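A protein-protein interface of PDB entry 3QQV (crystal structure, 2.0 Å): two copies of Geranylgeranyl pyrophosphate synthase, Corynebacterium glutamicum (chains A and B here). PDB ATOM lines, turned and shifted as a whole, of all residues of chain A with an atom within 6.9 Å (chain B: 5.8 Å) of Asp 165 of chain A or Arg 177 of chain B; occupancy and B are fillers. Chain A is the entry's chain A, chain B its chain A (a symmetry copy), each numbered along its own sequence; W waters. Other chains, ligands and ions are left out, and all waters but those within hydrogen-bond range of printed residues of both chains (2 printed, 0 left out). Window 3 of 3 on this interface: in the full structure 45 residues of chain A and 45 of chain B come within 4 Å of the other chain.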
ATOM      1  N   PHE A  32       8.778  16.235   7.239  1.00  0.00           N
ATOM      2  CA  PHE A  32       8.173  16.297   8.544  1.00  0.00           C
ATOM      3  C   PHE A  32       6.716  16.693   8.493  1.00  0.00           C
ATOM      4  O   PHE A  32       5.934  16.099   9.108  1.00  0.00           O
ATOM      5  CB  PHE A  32       8.924  17.261   9.429  1.00  0.00           C
ATOM      6  CG  PHE A  32       8.389  17.369  10.816  1.00  0.00           C
ATOM      7  CD1 PHE A  32       7.476  18.301  11.126  1.00  0.00           C
ATOM      8  CD2 PHE A  32       8.813  16.540  11.803  1.00  0.00           C
ATOM      9  CE1 PHE A  32       7.027  18.394  12.349  1.00  0.00           C
ATOM     10  CE2 PHE A  32       8.348  16.655  13.027  1.00  0.00           C
ATOM     11  CZ  PHE A  32       7.461  17.575  13.306  1.00  0.00           C
ATOM     12  N   SER A  89      19.521  12.615  10.517  1.00  0.00           N
ATOM     13  CA  SER A  89      19.283  13.062  11.892  1.00  0.00           C
ATOM     14  C   SER A  89      19.880  14.442  12.190  1.00  0.00           C
ATOM     15  O   SER A  89      19.233  15.283  12.833  1.00  0.00           O
ATOM     16  CB  SER A  89      19.831  12.034  12.867  1.00  0.00           C
ATOM     17  OG  SER A  89      19.229  10.773  12.646  1.00  0.00           O
ATOM     18  N   ASP A  92      17.823  17.087  10.170  1.00  0.00           N
ATOM     19  CA  ASP A  92      16.532  17.345  10.822  1.00  0.00           C
ATOM     20  C   ASP A  92      16.691  18.230  12.052  1.00  0.00           C
ATOM     21  O   ASP A  92      15.860  19.106  12.288  1.00  0.00           O
ATOM     22  CB  ASP A  92      15.835  16.040  11.229  1.00  0.00           C
ATOM     23  CG  ASP A  92      15.176  15.330  10.057  1.00  0.00           C
ATOM     24  OD1 ASP A  92      15.048  15.930   8.966  1.00  0.00           O
ATOM     25  OD2 ASP A  92      14.790  14.156  10.228  1.00  0.00           O
ATOM     26  N   VAL A 157       5.970  23.453  19.150  1.00  0.00           N
ATOM     27  CA  VAL A 157       5.838  22.055  19.542  1.00  0.00           C
ATOM     28  C   VAL A 157       6.478  21.114  18.500  1.00  0.00           C
ATOM     29  O   VAL A 157       7.095  20.092  18.841  1.00  0.00           O
ATOM     30  CB  VAL A 157       4.332  21.758  19.819  1.00  0.00           C
ATOM     31  CG1 VAL A 157       3.924  20.371  19.417  1.00  0.00           C
ATOM     32  CG2 VAL A 157       4.030  22.025  21.292  1.00  0.00           C
ATOM     33  N   GLU A 160      10.454  21.059  18.680  1.00  0.00           N
ATOM     34  CA  GLU A 160      10.899  20.127  19.709  1.00  0.00           C
ATOM     35  C   GLU A 160      10.789  18.693  19.231  1.00  0.00           C
ATOM     36  O   GLU A 160      11.728  17.918  19.403  1.00  0.00           O
ATOM     37  CB  GLU A 160      10.102  20.301  21.011  1.00  0.00           C
ATOM     38  CG  GLU A 160       9.792  21.740  21.401  1.00  0.00           C
ATOM     39  CD  GLU A 160      10.900  22.429  22.160  1.00  0.00           C
ATOM     40  OE1 GLU A 160      11.974  21.816  22.307  1.00  0.00           O
ATOM     41  OE2 GLU A 160      10.699  23.597  22.593  1.00  0.00           O
ATOM     42  N   ASP A 161       9.649  18.346  18.627  1.00  0.00           N
ATOM     43  CA  ASP A 161       9.441  16.982  18.094  1.00  0.00           C
ATOM     44  C   ASP A 161      10.465  16.615  17.011  1.00  0.00           C
ATOM     45  O   ASP A 161      11.034  15.525  17.042  1.00  0.00           O
ATOM     46  CB  ASP A 161       8.035  16.810  17.501  1.00  0.00           C
ATOM     47  CG  ASP A 161       6.937  16.846  18.545  1.00  0.00           C
ATOM     48  OD1 ASP A 161       7.219  16.695  19.758  1.00  0.00           O
ATOM     49  OD2 ASP A 161       5.771  17.024  18.128  1.00  0.00           O
ATOM     50  N   MET A 162      10.703  17.541  16.084  1.00  0.00           N
ATOM     51  CA  MET A 162      11.624  17.319  14.957  1.00  0.00           C
ATOM     52  C   MET A 162      13.056  17.045  15.422  1.00  0.00           C
ATOM     53  O   MET A 162      13.734  16.156  14.879  1.00  0.00           O
ATOM     54  CB  MET A 162      11.602  18.494  13.982  1.00  0.00           C
ATOM     55  CG  MET A 162      12.127  18.112  12.592  1.00  0.00           C
ATOM     56  SD  MET A 162      11.936  19.554  11.359  1.00  0.00           S
ATOM     57  CE  MET A 162      12.782  18.730   9.818  1.00  0.00           C
ATOM     58  N   LEU A 163      13.496  17.801  16.429  1.00  0.00           N
ATOM     59  CA  LEU A 163      14.730  17.503  17.147  1.00  0.00           C
ATOM     60  C   LEU A 163      14.676  16.151  17.878  1.00  0.00           C
ATOM     61  O   LEU A 163      15.516  15.289  17.636  1.00  0.00           O
ATOM     62  CB  LEU A 163      15.080  18.630  18.141  1.00  0.00           C
ATOM     63  CG  LEU A 163      16.345  18.382  18.972  1.00  0.00           C
ATOM     64  CD1 LEU A 163      17.582  18.458  18.092  1.00  0.00           C
ATOM     65  CD2 LEU A 163      16.467  19.326  20.168  1.00  0.00           C
ATOM     66  N   GLN A 164      13.705  15.970  18.774  1.00  0.00           N
ATOM     67  CA  GLN A 164      13.645  14.754  19.608  1.00  0.00           C
ATOM     68  C   GLN A 164      13.480  13.441  18.830  1.00  0.00           C
ATOM     69  O   GLN A 164      14.048  12.413  19.219  1.00  0.00           O
ATOM     70  CB  GLN A 164      12.564  14.856  20.699  1.00  0.00           C
ATOM     71  CG  GLN A 164      12.789  15.919  21.784  1.00  0.00           C
ATOM     72  CD  GLN A 164      14.178  15.904  22.390  1.00  0.00           C
ATOM     73  OE1 GLN A 164      14.746  14.846  22.659  1.00  0.00           O
ATOM     74  NE2 GLN A 164      14.725  17.088  22.624  1.00  0.00           N
ATOM     75  N   ASP A 165      12.714  13.479  17.740  1.00  0.00           N
ATOM     76  CA  ASP A 165      12.486  12.285  16.913  1.00  0.00           C
ATOM     77  C   ASP A 165      13.399  12.243  15.683  1.00  0.00           C
ATOM     78  O   ASP A 165      13.109  11.514  14.731  1.00  0.00           O
ATOM     79  CB  ASP A 165      11.020  12.206  16.442  1.00  0.00           C
ATOM     80  CG  ASP A 165      10.027  12.103  17.588  1.00  0.00           C
ATOM     81  OD1 ASP A 165      10.325  11.444  18.605  1.00  0.00           O
ATOM     82  OD2 ASP A 165       8.924  12.676  17.458  1.00  0.00           O
ATOM     83  N   SER A 166      14.484  13.026  15.695  1.00  0.00           N
ATOM     84  CA  SER A 166      15.408  13.119  14.555  1.00  0.00           C
ATOM     85  C   SER A 166      16.170  11.816  14.283  1.00  0.00           C
ATOM     86  O   SER A 166      16.585  11.568  13.151  1.00  0.00           O
ATOM     87  CB  SER A 166      16.416  14.264  14.753  1.00  0.00           C
ATOM     88  OG  SER A 166      17.165  14.062  15.940  1.00  0.00           O
ATOM     89  N   GLY A 167      16.340  10.997  15.316  1.00  0.00           N
ATOM     90  CA  GLY A 167      17.152   9.789  15.229  1.00  0.00           C
ATOM     91  C   GLY A 167      18.572  10.024  15.730  1.00  0.00           C
ATOM     92  O   GLY A 167      19.419   9.134  15.632  1.00  0.00           O
ATOM     93  N   LEU A 168      18.835  11.231  16.241  1.00  0.00           N
ATOM     94  CA  LEU A 168      20.090  11.525  16.934  1.00  0.00           C
ATOM     95  C   LEU A 168      20.134  10.639  18.162  1.00  0.00           C
ATOM     96  O   LEU A 168      19.109  10.436  18.814  1.00  0.00           O
ATOM     97  CB  LEU A 168      20.177  13.007  17.357  1.00  0.00           C
ATOM     98  CG  LEU A 168      20.510  14.121  16.355  1.00  0.00           C
ATOM     99  CD1 LEU A 168      20.473  15.477  17.060  1.00  0.00           C
ATOM    100  CD2 LEU A 168      21.860  13.915  15.662  1.00  0.00           C
ATOM    101  N   LEU A 173      21.706  13.991  21.787  1.00  0.00           N
ATOM    102  CA  LEU A 173      20.596  14.777  22.327  1.00  0.00           C
ATOM    103  C   LEU A 173      20.915  15.402  23.679  1.00  0.00           C
ATOM    104  O   LEU A 173      20.523  16.544  23.943  1.00  0.00           O
ATOM    105  CB  LEU A 173      19.313  13.950  22.421  1.00  0.00           C
ATOM    106  CG  LEU A 173      18.573  13.689  21.108  1.00  0.00           C
ATOM    107  CD1 LEU A 173      17.446  12.699  21.354  1.00  0.00           C
ATOM    108  CD2 LEU A 173      18.039  14.984  20.515  1.00  0.00           C
ATOM    109  N   GLN B 164      12.927  17.486  29.753  1.00  0.00           N
ATOM    110  CA  GLN B 164      14.246  17.078  29.232  1.00  0.00           C
ATOM    111  C   GLN B 164      15.390  17.129  30.254  1.00  0.00           C
ATOM    112  O   GLN B 164      16.284  16.274  30.229  1.00  0.00           O
ATOM    113  CB  GLN B 164      14.636  17.867  27.969  1.00  0.00           C
ATOM    114  CG  GLN B 164      13.768  17.633  26.725  1.00  0.00           C
ATOM    115  CD  GLN B 164      13.525  16.171  26.403  1.00  0.00           C
ATOM    116  OE1 GLN B 164      14.425  15.337  26.500  1.00  0.00           O
ATOM    117  NE2 GLN B 164      12.301  15.859  26.001  1.00  0.00           N
ATOM    118  N   ALA B 172      14.148   6.220  29.653  1.00  0.00           N
ATOM    119  CA  ALA B 172      12.848   6.725  30.075  1.00  0.00           C
ATOM    120  C   ALA B 172      12.342   7.838  29.165  1.00  0.00           C
ATOM    121  O   ALA B 172      11.172   7.831  28.776  1.00  0.00           O
ATOM    122  CB  ALA B 172      12.879   7.179  31.525  1.00  0.00           C
ATOM    123  N   LEU B 173      13.227   8.766  28.805  1.00  0.00           N
ATOM    124  CA  LEU B 173      12.875   9.863  27.902  1.00  0.00           C
ATOM    125  C   LEU B 173      12.446   9.380  26.522  1.00  0.00           C
ATOM    126  O   LEU B 173      11.518   9.940  25.929  1.00  0.00           O
ATOM    127  CB  LEU B 173      14.016  10.873  27.772  1.00  0.00           C
ATOM    128  CG  LEU B 173      14.220  11.826  28.952  1.00  0.00           C
ATOM    129  CD1 LEU B 173      15.502  12.617  28.744  1.00  0.00           C
ATOM    130  CD2 LEU B 173      13.028  12.756  29.116  1.00  0.00           C
ATOM    131  N   ALA B 174      13.101   8.334  26.026  1.00  0.00           N
ATOM    132  CA  ALA B 174      12.717   7.741  24.750  1.00  0.00           C
ATOM    133  C   ALA B 174      11.320   7.108  24.821  1.00  0.00           C
ATOM    134  O   ALA B 174      10.542   7.221  23.872  1.00  0.00           O
ATOM    135  CB  ALA B 174      13.769   6.741  24.258  1.00  0.00           C
ATOM    136  N   ARG B 175      11.003   6.481  25.955  1.00  0.00           N
ATOM    137  CA  ARG B 175       9.670   5.928  26.178  1.00  0.00           C
ATOM    138  C   ARG B 175       8.555   6.992  26.264  1.00  0.00           C
ATOM    139  O   ARG B 175       7.420   6.705  25.897  1.00  0.00           O
ATOM    140  CB  ARG B 175       9.650   5.034  27.419  1.00  0.00           C
ATOM    141  CG  ARG B 175      10.365   3.708  27.216  1.00  0.00           C
ATOM    142  CD  ARG B 175       9.982   2.704  28.279  1.00  0.00           C
ATOM    143  NE  ARG B 175      10.227   3.181  29.640  1.00  0.00           N
ATOM    144  CZ  ARG B 175      11.360   2.977  30.308  1.00  0.00           C
ATOM    145  NH1 ARG B 175      11.494   3.434  31.542  1.00  0.00           N
ATOM    146  NH2 ARG B 175      12.356   2.308  29.742  1.00  0.00           N
ATOM    147  N   THR B 176       8.889   8.208  26.716  1.00  0.00           N
ATOM    148  CA  THR B 176       7.903   9.298  26.843  1.00  0.00           C
ATOM    149  C   THR B 176       7.401   9.832  25.509  1.00  0.00           C
ATOM    150  O   THR B 176       6.353  10.477  25.470  1.00  0.00           O
ATOM    151  CB  THR B 176       8.429  10.537  27.654  1.00  0.00           C
ATOM    152  OG1 THR B 176       9.438  11.238  26.909  1.00  0.00           O
ATOM    153  CG2 THR B 176       8.940  10.155  29.034  1.00  0.00           C
ATOM    154  N   ARG B 177       8.131   9.565  24.428  1.00  0.00           N
ATOM    155  CA  ARG B 177       7.878  10.215  23.134  1.00  0.00           C
ATOM    156  C   ARG B 177       6.448  10.085  22.611  1.00  0.00           C
ATOM    157  O   ARG B 177       5.858  11.067  22.177  1.00  0.00           O
ATOM    158  CB  ARG B 177       8.863   9.718  22.064  1.00  0.00           C
ATOM    159  CG  ARG B 177      10.302  10.210  22.217  1.00  0.00           C
ATOM    160  CD  ARG B 177      10.393  11.724  22.342  1.00  0.00           C
ATOM    161  NE  ARG B 177       9.832  12.420  21.186  1.00  0.00           N
ATOM    162  CZ  ARG B 177       9.288  13.630  21.245  1.00  0.00           C
ATOM    163  NH1 ARG B 177       9.227  14.272  22.402  1.00  0.00           N
ATOM    164  NH2 ARG B 177       8.805  14.193  20.151  1.00  0.00           N
ATOM    165  N   ASP B 178       5.888   8.881  22.654  1.00  0.00           N
ATOM    166  CA  ASP B 178       4.540   8.656  22.098  1.00  0.00           C
ATOM    167  C   ASP B 178       3.474   9.477  22.809  1.00  0.00           C
ATOM    168  O   ASP B 178       2.672  10.162  22.161  1.00  0.00           O
ATOM    169  CB  ASP B 178       4.182   7.158  22.103  1.00  0.00           C
ATOM    170  CG  ASP B 178       4.973   6.362  21.067  1.00  0.00           C
ATOM    171  OD1 ASP B 178       5.498   6.966  20.104  1.00  0.00           O
ATOM    172  OD2 ASP B 178       5.063   5.124  21.214  1.00  0.00           O
ATOM    173  N   ALA B 179       3.489   9.446  24.139  1.00  0.00           N
ATOM    174  CA  ALA B 179       2.531  10.217  24.914  1.00  0.00           C
ATOM    175  C   ALA B 179       2.745  11.713  24.737  1.00  0.00           C
ATOM    176  O   ALA B 179       1.790  12.454  24.531  1.00  0.00           O
ATOM    177  CB  ALA B 179       2.610   9.845  26.379  1.00  0.00           C
ATOM    178  N   TRP B 180       4.009  12.136  24.800  1.00  0.00           N
ATOM    179  CA  TRP B 180       4.379  13.550  24.773  1.00  0.00           C
ATOM    180  C   TRP B 180       4.133  14.190  23.398  1.00  0.00           C
ATOM    181  O   TRP B 180       3.588  15.298  23.311  1.00  0.00           O
ATOM    182  CB  TRP B 180       5.848  13.694  25.194  1.00  0.00           C
ATOM    183  CG  TRP B 180       6.278  15.100  25.501  1.00  0.00           C
ATOM    184  CD1 TRP B 180       6.972  15.937  24.679  1.00  0.00           C
ATOM    185  CD2 TRP B 180       6.065  15.818  26.721  1.00  0.00           C
ATOM    186  NE1 TRP B 180       7.203  17.140  25.308  1.00  0.00           N
ATOM    187  CE2 TRP B 180       6.645  17.101  26.559  1.00  0.00           C
ATOM    188  CE3 TRP B 180       5.452  15.504  27.941  1.00  0.00           C
ATOM    189  CZ2 TRP B 180       6.629  18.067  27.569  1.00  0.00           C
ATOM    190  CZ3 TRP B 180       5.427  16.473  28.948  1.00  0.00           C
ATOM    191  CH2 TRP B 180       6.019  17.736  28.759  1.00  0.00           C
ATOM    192  N   ARG B 181       4.541  13.497  22.338  1.00  0.00           N
ATOM    193  CA  ARG B 181       4.299  13.935  20.962  1.00  0.00           C
ATOM    194  C   ARG B 181       2.792  13.968  20.694  1.00  0.00           C
ATOM    195  O   ARG B 181       2.283  14.950  20.161  1.00  0.00           O
ATOM    196  CB  ARG B 181       4.985  13.000  19.963  1.00  0.00           C
ATOM    197  CG  ARG B 181       4.747  13.308  18.478  1.00  0.00           C
ATOM    198  CD  ARG B 181       5.090  12.122  17.549  1.00  0.00           C
ATOM    199  NE  ARG B 181       6.343  11.469  17.931  1.00  0.00           N
ATOM    200  CZ  ARG B 181       6.457  10.207  18.339  1.00  0.00           C
ATOM    201  NH1 ARG B 181       5.395   9.419  18.399  1.00  0.00           N
ATOM    202  NH2 ARG B 181       7.645   9.727  18.679  1.00  0.00           N
ATOM    203  N   GLY B 182       2.101  12.896  21.078  1.00  0.00           N
ATOM    204  CA  GLY B 182       0.649  12.806  20.924  1.00  0.00           C
ATOM    205  C   GLY B 182      -0.069  13.961  21.583  1.00  0.00           C
ATOM    206  O   GLY B 182      -0.753  14.725  20.913  1.00  0.00           O
ATOM    207  N   ARG B 184       0.736  17.010  22.788  1.00  0.00           N
ATOM    208  CA  ARG B 184       0.939  18.411  22.448  1.00  0.00           C
ATOM    209  C   ARG B 184       0.337  18.804  21.078  1.00  0.00           C
ATOM    210  O   ARG B 184      -0.164  19.916  20.919  1.00  0.00           O
ATOM    211  CB  ARG B 184       2.426  18.756  22.554  1.00  0.00           C
ATOM    212  CG  ARG B 184       2.895  18.948  23.997  1.00  0.00           C
ATOM    213  CD  ARG B 184       4.287  18.359  24.219  1.00  0.00           C
ATOM    214  NE  ARG B 184       5.313  18.963  23.365  1.00  0.00           N
ATOM    215  CZ  ARG B 184       5.875  18.384  22.307  1.00  0.00           C
ATOM    216  NH1 ARG B 184       5.528  17.153  21.929  1.00  0.00           N
ATOM    217  NH2 ARG B 184       6.794  19.050  21.614  1.00  0.00           N
HETATM  218  O   HOH W   1       3.375  17.085  19.328  1.00  0.00           O
HETATM  219  O   HOH W   2       9.080  16.900  22.247  1.00  0.00           O
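OD1 of Asp 178 of chain B is in salt-bridge range of NH1 of Arg 181 of chain B, 3.0 Å away.
O of Trp 180 of chain B lies within hydrogen-bond range of NH1 of Arg 184 of chain B (3.0 Å).
Asp 165 of chain A touches just these residues of chain B: Arg 177 and Arg 181.
Arg 177 of chain B touches just these residues of chain A: Asp 161, Gln 164 and Asp 165.
Of the printed residues of chain A, Arg 181 of chain B touches Asp 161 and Asp 165.
Of the printed residues of chain A, Arg 184 of chain B touches Val 157, Glu 160 and Asp 161.
Asp 92 of chain A touches none of the printed residues of chain B.
Gly 167 of chain A touches none of the printed residues of chain B.
The nearest printed residue of chain B that does not touch Asp 165 of chain A is Asp 178 of chain B (6.5 Å).
Gln 164 of chain A touches its own counterpart, Gln 164 of chain B.
2 positions are printed for both chains.
Of the 9 pairs that touch across the chains among the printed residues, 1 has its exchanged pair printed and touching as well.
Water W1 lies within hydrogen-bond range of O of Arg 181 of chain B, OD2 of Asp 161 of chain A and NH1 of Arg 184 of chain B.
Water W2 lies within hydrogen-bond range of NH1 of Arg 177 of chain B (2.6 Å), OD1 of Asp 161 of chain A (3.1 Å) and NH2 of Arg 184 of chain B (3.2 Å).
Among the printed residues, merely in contact across the chains: Glu 160 of chain A with Arg 184 of chain B, Asp 161 of chain A with Arg 181 of chain B, Gln 164 of chain A with Gln 164 of chain B and Gln 164 of chain A with Arg 177 of chain B.
O of Val 157 of chain A sits at hydrogen-bond distance from NH2 of Arg 184 of chain B, at 3.0 Å.
The side-chain carboxylate (OD1) of Asp 161 of chain A is in salt-bridge range of the guanidinium group (NH2) of Arg 177 of chain B (3.0 Å).
NH1 of Arg 184 of chain B is in salt-bridge range of OD1 of Asp 161 of chain A (2.8 Å).
The side-chain carboxylate (OD1) of Asp 165 of chain A is in salt-bridge range of the guanidinium group (NE) of Arg 177 of chain B, at 2.8 Å.
OD2 of Asp 165 of chain A is in salt-bridge range of NE of Arg 181 of chain B (2.9 Å).
Of the 13 printed residues of chain B, 4 touch a printed residue of chain A.
Printed residues of chain B that touch a printed residue of chain A: Gln 164, Arg 177, Arg 181 and Arg 184.
Of the 14 printed residues of chain A, 5 touch a printed residue of chain B.
Among the printed residues, 9 pairs touch across the chains.
Among the printed residues, Asp or Glu carboxylates within 4 Å of a Lys or Arg side-chain nitrogen of the other chain: Asp 161 of chain A with Arg 177 of chain B (3.0 Å), Asp 161 of chain A with Arg 184 of chain B (2.8 Å), Asp 165 of chain A with Arg 177 of chain B (2.8 Å) and Asp 165 of chain A with Arg 181 of chain B (2.9 Å).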
